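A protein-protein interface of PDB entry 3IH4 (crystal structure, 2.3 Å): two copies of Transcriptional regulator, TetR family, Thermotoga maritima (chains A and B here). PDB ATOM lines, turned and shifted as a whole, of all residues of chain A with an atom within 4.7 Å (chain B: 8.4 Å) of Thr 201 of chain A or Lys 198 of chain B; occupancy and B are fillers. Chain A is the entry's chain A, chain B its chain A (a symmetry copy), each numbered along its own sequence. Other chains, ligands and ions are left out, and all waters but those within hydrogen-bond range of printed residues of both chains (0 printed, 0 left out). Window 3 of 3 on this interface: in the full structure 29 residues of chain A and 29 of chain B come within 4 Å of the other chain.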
ATOM      1  N   LEU A 141     -14.333 -11.225   7.248  1.00  0.00           N
ATOM      2  CA  LEU A 141     -13.924  -9.829   7.021  1.00  0.00           C
ATOM      3  C   LEU A 141     -12.851  -9.396   8.058  1.00  0.00           C
ATOM      4  O   LEU A 141     -12.930  -9.768   9.237  1.00  0.00           O
ATOM      5  CB  LEU A 141     -15.182  -8.953   7.145  1.00  0.00           C
ATOM      6  CG  LEU A 141     -15.379  -7.663   6.331  1.00  0.00           C
ATOM      7  CD1 LEU A 141     -15.622  -7.948   4.858  1.00  0.00           C
ATOM      8  CD2 LEU A 141     -16.557  -6.880   6.895  1.00  0.00           C
ATOM      9  N   ASP A 142     -11.858  -8.617   7.619  1.00  0.00           N
ATOM     10  CA  ASP A 142     -10.834  -8.058   8.526  1.00  0.00           C
ATOM     11  C   ASP A 142     -11.296  -6.742   9.118  1.00  0.00           C
ATOM     12  O   ASP A 142     -10.963  -5.671   8.601  1.00  0.00           O
ATOM     13  CB  ASP A 142      -9.508  -7.783   7.781  1.00  0.00           C
ATOM     14  CG  ASP A 142      -8.481  -8.876   7.950  1.00  0.00           C
ATOM     15  OD1 ASP A 142      -8.776  -9.942   8.562  1.00  0.00           O
ATOM     16  OD2 ASP A 142      -7.354  -8.644   7.448  1.00  0.00           O
ATOM     17  N   LEU A 143     -12.024  -6.803  10.221  1.00  0.00           N
ATOM     18  CA  LEU A 143     -12.638  -5.605  10.738  1.00  0.00           C
ATOM     19  C   LEU A 143     -11.599  -4.730  11.415  1.00  0.00           C
ATOM     20  O   LEU A 143     -10.642  -5.232  11.994  1.00  0.00           O
ATOM     21  CB  LEU A 143     -13.805  -5.924  11.670  1.00  0.00           C
ATOM     22  CG  LEU A 143     -15.106  -6.344  10.967  1.00  0.00           C
ATOM     23  CD1 LEU A 143     -16.179  -6.551  11.999  1.00  0.00           C
ATOM     24  CD2 LEU A 143     -15.551  -5.325   9.924  1.00  0.00           C
ATOM     25  N   ALA A 144     -11.785  -3.419  11.303  1.00  0.00           N
ATOM     26  CA  ALA A 144     -10.916  -2.464  11.943  1.00  0.00           C
ATOM     27  C   ALA A 144     -10.928  -2.769  13.429  1.00  0.00           C
ATOM     28  O   ALA A 144     -12.005  -2.890  14.021  1.00  0.00           O
ATOM     29  CB  ALA A 144     -11.402  -1.048  11.683  1.00  0.00           C
ATOM     30  N   LYS A 197     -17.019  -0.329   3.281  1.00  0.00           N
ATOM     31  CA  LYS A 197     -15.989  -1.358   3.317  1.00  0.00           C
ATOM     32  C   LYS A 197     -14.646  -0.779   3.776  1.00  0.00           C
ATOM     33  O   LYS A 197     -14.012  -1.320   4.687  1.00  0.00           O
ATOM     34  CB  LYS A 197     -15.810  -2.035   1.944  1.00  0.00           C
ATOM     35  CG  LYS A 197     -14.892  -3.294   1.983  1.00  0.00           C
ATOM     36  CD  LYS A 197     -15.045  -4.226   0.763  1.00  0.00           C
ATOM     37  CE  LYS A 197     -14.306  -5.616   1.026  1.00  0.00           C
ATOM     38  NZ  LYS A 197     -14.405  -6.682  -0.065  1.00  0.00           N
ATOM     39  N   LYS A 198     -14.216   0.312   3.144  1.00  0.00           N
ATOM     40  CA  LYS A 198     -12.938   0.960   3.497  1.00  0.00           C
ATOM     41  C   LYS A 198     -12.877   1.403   4.957  1.00  0.00           C
ATOM     42  O   LYS A 198     -11.898   1.154   5.617  1.00  0.00           O
ATOM     43  CB  LYS A 198     -12.629   2.147   2.565  1.00  0.00           C
ATOM     44  CG  LYS A 198     -11.321   2.834   2.930  1.00  0.00           C
ATOM     45  CD  LYS A 198     -11.085   4.122   2.183  1.00  0.00           C
ATOM     46  CE  LYS A 198      -9.825   4.818   2.658  1.00  0.00           C
ATOM     47  NZ  LYS A 198      -9.588   5.997   1.766  1.00  0.00           N
ATOM     48  N   GLY A 199     -13.928   2.066   5.441  1.00  0.00           N
ATOM     49  CA  GLY A 199     -13.988   2.590   6.797  1.00  0.00           C
ATOM     50  C   GLY A 199     -14.127   1.532   7.869  1.00  0.00           C
ATOM     51  O   GLY A 199     -13.811   1.744   9.027  1.00  0.00           O
ATOM     52  N   MET A 200     -14.585   0.373   7.453  1.00  0.00           N
ATOM     53  CA  MET A 200     -14.958  -0.687   8.349  1.00  0.00           C
ATOM     54  C   MET A 200     -13.862  -1.743   8.479  1.00  0.00           C
ATOM     55  O   MET A 200     -13.858  -2.509   9.437  1.00  0.00           O
ATOM     56  CB  MET A 200     -16.198  -1.318   7.754  1.00  0.00           C
ATOM     57  CG  MET A 200     -17.043  -2.070   8.669  1.00  0.00           C
ATOM     58  SD  MET A 200     -18.750  -2.354   7.762  1.00  0.00           S
ATOM     59  CE  MET A 200     -19.740  -0.726   8.167  1.00  0.00           C
ATOM     60  N   THR A 201     -12.943  -1.785   7.521  1.00  0.00           N
ATOM     61  CA  THR A 201     -11.961  -2.862   7.458  1.00  0.00           C
ATOM     62  C   THR A 201     -10.506  -2.357   7.563  1.00  0.00           C
ATOM     63  O   THR A 201     -10.246  -1.149   7.467  1.00  0.00           O
ATOM     64  CB  THR A 201     -12.150  -3.705   6.170  1.00  0.00           C
ATOM     65  OG1 THR A 201     -11.725  -2.958   5.031  1.00  0.00           O
ATOM     66  CG2 THR A 201     -13.604  -4.110   5.973  1.00  0.00           C
ATOM     67  N   LYS A 202      -9.576  -3.293   7.786  1.00  0.00           N
ATOM     68  CA  LYS A 202      -8.134  -2.989   7.899  1.00  0.00           C
ATOM     69  C   LYS A 202      -7.518  -2.592   6.563  1.00  0.00           C
ATOM     70  O   LYS A 202      -6.625  -1.741   6.470  1.00  0.00           O
ATOM     71  CB  LYS A 202      -7.359  -4.183   8.471  1.00  0.00           C
ATOM     72  CG  LYS A 202      -7.509  -4.339   9.986  1.00  0.00           C
ATOM     73  CD  LYS A 202      -6.263  -4.972  10.674  1.00  0.00           C
ATOM     74  CE  LYS A 202      -6.243  -6.479  10.612  1.00  0.00           C
ATOM     75  NZ  LYS A 202      -7.333  -7.072  11.457  1.00  0.00           N
ATOM     76  OXT LYS A 202      -7.913  -3.113   5.527  1.00  0.00           O
ATOM     77  N   PHE B  81     -17.402  16.032  11.363  1.00  0.00           N
ATOM     78  CA  PHE B  81     -17.723  14.780  12.051  1.00  0.00           C
ATOM     79  C   PHE B  81     -17.864  14.994  13.545  1.00  0.00           C
ATOM     80  O   PHE B  81     -18.828  14.568  14.145  1.00  0.00           O
ATOM     81  CB  PHE B  81     -16.668  13.695  11.770  1.00  0.00           C
ATOM     82  CG  PHE B  81     -16.663  13.238  10.348  1.00  0.00           C
ATOM     83  CD1 PHE B  81     -15.802  13.797   9.429  1.00  0.00           C
ATOM     84  CD2 PHE B  81     -17.564  12.297   9.914  1.00  0.00           C
ATOM     85  CE1 PHE B  81     -15.829  13.409   8.104  1.00  0.00           C
ATOM     86  CE2 PHE B  81     -17.600  11.912   8.606  1.00  0.00           C
ATOM     87  CZ  PHE B  81     -16.722  12.475   7.697  1.00  0.00           C
ATOM     88  N   ASP B 142     -10.110  16.157   2.859  1.00  0.00           N
ATOM     89  CA  ASP B 142      -9.368  15.444   1.798  1.00  0.00           C
ATOM     90  C   ASP B 142     -10.143  14.235   1.314  1.00  0.00           C
ATOM     91  O   ASP B 142      -9.916  13.116   1.782  1.00  0.00           O
ATOM     92  CB  ASP B 142      -8.001  14.933   2.310  1.00  0.00           C
ATOM     93  CG  ASP B 142      -6.846  15.837   1.952  1.00  0.00           C
ATOM     94  OD1 ASP B 142      -7.053  16.946   1.384  1.00  0.00           O
ATOM     95  OD2 ASP B 142      -5.706  15.407   2.257  1.00  0.00           O
ATOM     96  N   LEU B 143     -11.027  14.438   0.351  1.00  0.00           N
ATOM     97  CA  LEU B 143     -11.917  13.370  -0.036  1.00  0.00           C
ATOM     98  C   LEU B 143     -11.176  12.340  -0.867  1.00  0.00           C
ATOM     99  O   LEU B 143     -10.259  12.678  -1.609  1.00  0.00           O
ATOM    100  CB  LEU B 143     -13.154  13.899  -0.759  1.00  0.00           C
ATOM    101  CG  LEU B 143     -14.224  14.526   0.149  1.00  0.00           C
ATOM    102  CD1 LEU B 143     -15.405  14.929  -0.687  1.00  0.00           C
ATOM    103  CD2 LEU B 143     -14.652  13.583   1.268  1.00  0.00           C
ATOM    104  N   ALA B 144     -11.562  11.079  -0.706  1.00  0.00           N
ATOM    105  CA  ALA B 144     -10.993   9.998  -1.471  1.00  0.00           C
ATOM    106  C   ALA B 144     -11.206  10.323  -2.937  1.00  0.00           C
ATOM    107  O   ALA B 144     -12.331  10.636  -3.338  1.00  0.00           O
ATOM    108  CB  ALA B 144     -11.663   8.684  -1.110  1.00  0.00           C
ATOM    109  N   VAL B 147     -14.398   9.603  -4.424  1.00  0.00           N
ATOM    110  CA  VAL B 147     -15.593  10.123  -3.719  1.00  0.00           C
ATOM    111  C   VAL B 147     -15.834  11.630  -3.971  1.00  0.00           C
ATOM    112  O   VAL B 147     -15.049  12.470  -3.522  1.00  0.00           O
ATOM    113  CB  VAL B 147     -15.452   9.927  -2.171  1.00  0.00           C
ATOM    114  CG1 VAL B 147     -16.547  10.680  -1.407  1.00  0.00           C
ATOM    115  CG2 VAL B 147     -15.464   8.472  -1.822  1.00  0.00           C
ATOM    116  N   VAL B 191     -18.306   5.525  16.591  1.00  0.00           N
ATOM    117  CA  VAL B 191     -17.582   4.576  15.733  1.00  0.00           C
ATOM    118  C   VAL B 191     -18.096   4.687  14.274  1.00  0.00           C
ATOM    119  O   VAL B 191     -17.311   4.774  13.341  1.00  0.00           O
ATOM    120  CB  VAL B 191     -17.730   3.120  16.243  1.00  0.00           C
ATOM    121  CG1 VAL B 191     -16.963   2.148  15.335  1.00  0.00           C
ATOM    122  CG2 VAL B 191     -17.307   2.979  17.715  1.00  0.00           C
ATOM    123  N   MET B 192     -19.408   4.738  14.089  1.00  0.00           N
ATOM    124  CA  MET B 192     -19.994   4.896  12.745  1.00  0.00           C
ATOM    125  C   MET B 192     -19.592   6.154  12.013  1.00  0.00           C
ATOM    126  O   MET B 192     -19.304   6.087  10.830  1.00  0.00           O
ATOM    127  CB  MET B 192     -21.509   4.808  12.781  1.00  0.00           C
ATOM    128  CG  MET B 192     -21.963   3.439  13.180  1.00  0.00           C
ATOM    129  SD  MET B 192     -23.921   3.244  13.225  1.00  0.00           S
ATOM    130  CE  MET B 192     -23.968   1.782  14.541  1.00  0.00           C
ATOM    131  N   LEU B 193     -19.598   7.299  12.684  1.00  0.00           N
ATOM    132  CA  LEU B 193     -19.010   8.508  12.101  1.00  0.00           C
ATOM    133  C   LEU B 193     -17.513   8.323  11.786  1.00  0.00           C
ATOM    134  O   LEU B 193     -17.016   8.854  10.796  1.00  0.00           O
ATOM    135  CB  LEU B 193     -19.255   9.740  12.981  1.00  0.00           C
ATOM    136  CG  LEU B 193     -20.682  10.306  12.872  1.00  0.00           C
ATOM    137  CD1 LEU B 193     -21.050  11.303  13.955  1.00  0.00           C
ATOM    138  CD2 LEU B 193     -20.969  10.908  11.483  1.00  0.00           C
ATOM    139  N   ARG B 194     -16.802   7.549  12.597  1.00  0.00           N
ATOM    140  CA  ARG B 194     -15.389   7.243  12.328  1.00  0.00           C
ATOM    141  C   ARG B 194     -15.197   6.336  11.152  1.00  0.00           C
ATOM    142  O   ARG B 194     -14.287   6.561  10.364  1.00  0.00           O
ATOM    143  CB  ARG B 194     -14.695   6.681  13.556  1.00  0.00           C
ATOM    144  CG  ARG B 194     -14.089   7.790  14.355  1.00  0.00           C
ATOM    145  CD  ARG B 194     -13.883   7.444  15.787  1.00  0.00           C
ATOM    146  NE  ARG B 194     -13.337   6.113  15.988  1.00  0.00           N
ATOM    147  CZ  ARG B 194     -13.522   5.437  17.118  1.00  0.00           C
ATOM    148  NH1 ARG B 194     -14.246   5.979  18.115  1.00  0.00           N
ATOM    149  NH2 ARG B 194     -13.012   4.214  17.260  1.00  0.00           N
ATOM    150  N   ILE B 195     -16.067   5.347  10.998  1.00  0.00           N
ATOM    151  CA  ILE B 195     -16.111   4.578   9.775  1.00  0.00           C
ATOM    152  C   ILE B 195     -16.347   5.499   8.547  1.00  0.00           C
ATOM    153  O   ILE B 195     -15.612   5.410   7.546  1.00  0.00           O
ATOM    154  CB  ILE B 195     -17.210   3.470   9.839  1.00  0.00           C
ATOM    155  CG1 ILE B 195     -16.883   2.426  10.939  1.00  0.00           C
ATOM    156  CG2 ILE B 195     -17.394   2.785   8.501  1.00  0.00           C
ATOM    157  CD1 ILE B 195     -17.979   1.401  11.166  1.00  0.00           C
ATOM    158  N   LEU B 196     -17.331   6.402   8.618  1.00  0.00           N
ATOM    159  CA  LEU B 196     -17.588   7.271   7.469  1.00  0.00           C
ATOM    160  C   LEU B 196     -16.361   8.123   7.146  1.00  0.00           C
ATOM    161  O   LEU B 196     -15.959   8.156   6.005  1.00  0.00           O
ATOM    162  CB  LEU B 196     -18.832   8.177   7.631  1.00  0.00           C
ATOM    163  CG  LEU B 196     -20.190   7.487   7.738  1.00  0.00           C
ATOM    164  CD1 LEU B 196     -21.290   8.566   7.945  1.00  0.00           C
ATOM    165  CD2 LEU B 196     -20.502   6.610   6.534  1.00  0.00           C
ATOM    166  N   LYS B 197     -15.800   8.815   8.138  1.00  0.00           N
ATOM    167  CA  LYS B 197     -14.630   9.653   7.911  1.00  0.00           C
ATOM    168  C   LYS B 197     -13.505   8.858   7.238  1.00  0.00           C
ATOM    169  O   LYS B 197     -12.953   9.296   6.224  1.00  0.00           O
ATOM    170  CB  LYS B 197     -14.105  10.268   9.223  1.00  0.00           C
ATOM    171  CG  LYS B 197     -13.005  11.351   9.009  1.00  0.00           C
ATOM    172  CD  LYS B 197     -12.785  12.277  10.223  1.00  0.00           C
ATOM    173  CE  LYS B 197     -11.873  13.523   9.817  1.00  0.00           C
ATOM    174  NZ  LYS B 197     -11.600  14.574  10.893  1.00  0.00           N
ATOM    175  N   LYS B 198     -13.168   7.700   7.803  1.00  0.00           N
ATOM    176  CA  LYS B 198     -12.099   6.848   7.247  1.00  0.00           C
ATOM    177  C   LYS B 198     -12.365   6.422   5.805  1.00  0.00           C
ATOM    178  O   LYS B 198     -11.486   6.509   4.984  1.00  0.00           O
ATOM    179  CB  LYS B 198     -11.844   5.612   8.130  1.00  0.00           C
ATOM    180  CG  LYS B 198     -10.755   4.715   7.557  1.00  0.00           C
ATOM    181  CD  LYS B 198     -10.620   3.395   8.272  1.00  0.00           C
ATOM    182  CE  LYS B 198      -9.599   2.500   7.599  1.00  0.00           C
ATOM    183  NZ  LYS B 198      -9.419   1.284   8.455  1.00  0.00           N
ATOM    184  N   GLY B 199     -13.581   5.957   5.517  1.00  0.00           N
ATOM    185  CA  GLY B 199     -13.962   5.472   4.200  1.00  0.00           C
ATOM    186  C   GLY B 199     -14.098   6.553   3.151  1.00  0.00           C
ATOM    187  O   GLY B 199     -14.026   6.307   1.960  1.00  0.00           O
ATOM    188  N   MET B 200     -14.272   7.767   3.622  1.00  0.00           N
ATOM    189  CA  MET B 200     -14.605   8.889   2.788  1.00  0.00           C
ATOM    190  C   MET B 200     -13.383   9.743   2.456  1.00  0.00           C
ATOM    191  O   MET B 200     -13.411  10.511   1.501  1.00  0.00           O
ATOM    192  CB  MET B 200     -15.598   9.715   3.576  1.00  0.00           C
ATOM    193  CG  MET B 200     -16.445  10.614   2.808  1.00  0.00           C
ATOM    194  SD  MET B 200     -17.898  11.175   3.989  1.00  0.00           S
ATOM    195  CE  MET B 200     -19.207   9.747   3.784  1.00  0.00           C
ATOM    196  N   THR B 201     -12.319   9.613   3.242  1.00  0.00           N
ATOM    197  CA  THR B 201     -11.171  10.504   3.120  1.00  0.00           C
ATOM    198  C   THR B 201      -9.865   9.757   2.776  1.00  0.00           C
ATOM    199  O   THR B 201      -9.803   8.521   2.844  1.00  0.00           O
ATOM    200  CB  THR B 201     -10.990  11.347   4.409  1.00  0.00           C
ATOM    201  OG1 THR B 201     -10.511  10.521   5.471  1.00  0.00           O
ATOM    202  CG2 THR B 201     -12.297  11.993   4.846  1.00  0.00           C
ATOM    203  N   LYS B 202      -8.840  10.523   2.384  1.00  0.00           N
ATOM    204  CA  LYS B 202      -7.512   9.978   2.031  1.00  0.00           C
ATOM    205  C   LYS B 202      -6.755   9.461   3.247  1.00  0.00           C
ATOM    206  O   LYS B 202      -6.018   8.467   3.199  1.00  0.00           O
ATOM    207  CB  LYS B 202      -6.652  11.028   1.317  1.00  0.00           C
ATOM    208  CG  LYS B 202      -7.030  11.231  -0.153  1.00  0.00           C
ATOM    209  CD  LYS B 202      -5.830  11.650  -1.052  1.00  0.00           C
ATOM    210  CE  LYS B 202      -5.541  13.130  -1.017  1.00  0.00           C
ATOM    211  NZ  LYS B 202      -6.642  13.915  -1.672  1.00  0.00           N
ATOM    212  OXT LYS B 202      -6.871  10.026   4.328  1.00  0.00           O
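Lys 198 of chain A touches Lys 198 of chain B.
Lys 198 of chain A touches Gly 199 of chain B (CD to O, 3.7 Å).
O of Ile 195 of chain B touches CA of Gly 199 of chain A, 3.3 Å away.
Lys 198 of chain B touches Gly 199 of chain A.
Gly 199 of chain B touches Gly 199 of chain A (N to CA, 3.6 Å).
Met 200 of chain A touches Ile 195 of chain B (N to CG2, 3.8 Å).
Of the printed residues of chain B, Lys 198 of chain A touches Lys 198, Gly 199 and Thr 201.
Of the printed residues of chain B, Met 200 of chain A touches Ile 195.
Thr 201 of chain A touches just one residue of chain B: Lys 198 (2.8 Å).
Of the printed residues of chain A, Ile 195 of chain B touches Gly 199 and Met 200.
Of chain A, only Lys 198, Gly 199 and Thr 201 come within 4 Å of Lys 198 of chain B.
Of the printed residues of chain A, Thr 201 of chain B touches Lys 198 (2.8 Å).
The nearest residue of chain A that does not touch Lys 198 of chain B is Ala 144 of chain A (4.4 Å).
The side-chain amino group of Lys 198 of chain B is in hydrogen-bond range of the backbone carbonyl oxygen of Thr 201 of chain A, at 2.8 Å.
The backbone carbonyl oxygen (O) of Thr 201 of chain B sits at hydrogen-bond distance from the side-chain amino group (NZ) of Lys 198 of chain A, at 2.8 Å.
Printed residues of chain B that touch a printed residue of chain A: Ile 195, Lys 198, Gly 199 and Thr 201.
Hydrophobic or aromatic side chains of chain B that line the printed part of chain A: Ile 195.
Along chain B the printed residues that touch a printed residue of chain A span positions 195 to 201.
Among the printed residues, 8 pairs touch across the chains.
Among the printed residues, no Asp or Glu carboxylate lies within 4 Å of a Lys or Arg side-chain nitrogen of the other chain.
Lys 198 of chain A touches its own counterpart, Lys 198 of chain B.
Lys 198 of chain A touches Gly 199 of chain B, and with the chains exchanged Gly 199 of chain A touches Lys 198 of chain B.
Lys 198 of chain A touches Thr 201 of chain B, and with the chains exchanged Thr 201 of chain A touches Lys 198 of chain B.
Gly 199 of chain B touches its own counterpart, Gly 199 of chain A.
Of the 8 pairs that touch across the chains among the printed residues, 6 have their exchanged pair printed and touching as well.
The backbone carbonyl oxygen (O) of Met 200 of chain A is in hydrogen-bond range of the backbone NH (N) of Ala 144 of chain A (2.9 Å).
The backbone carbonyl oxygen (O) of Lys 197 of chain A is in hydrogen-bond range of the side-chain hydroxyl (OG1) of Thr 201 of chain A, 2.8 Å away.
O of Lys 197 of chain B is in hydrogen-bond range of OG1 of Thr 201 of chain B (2.8 Å).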
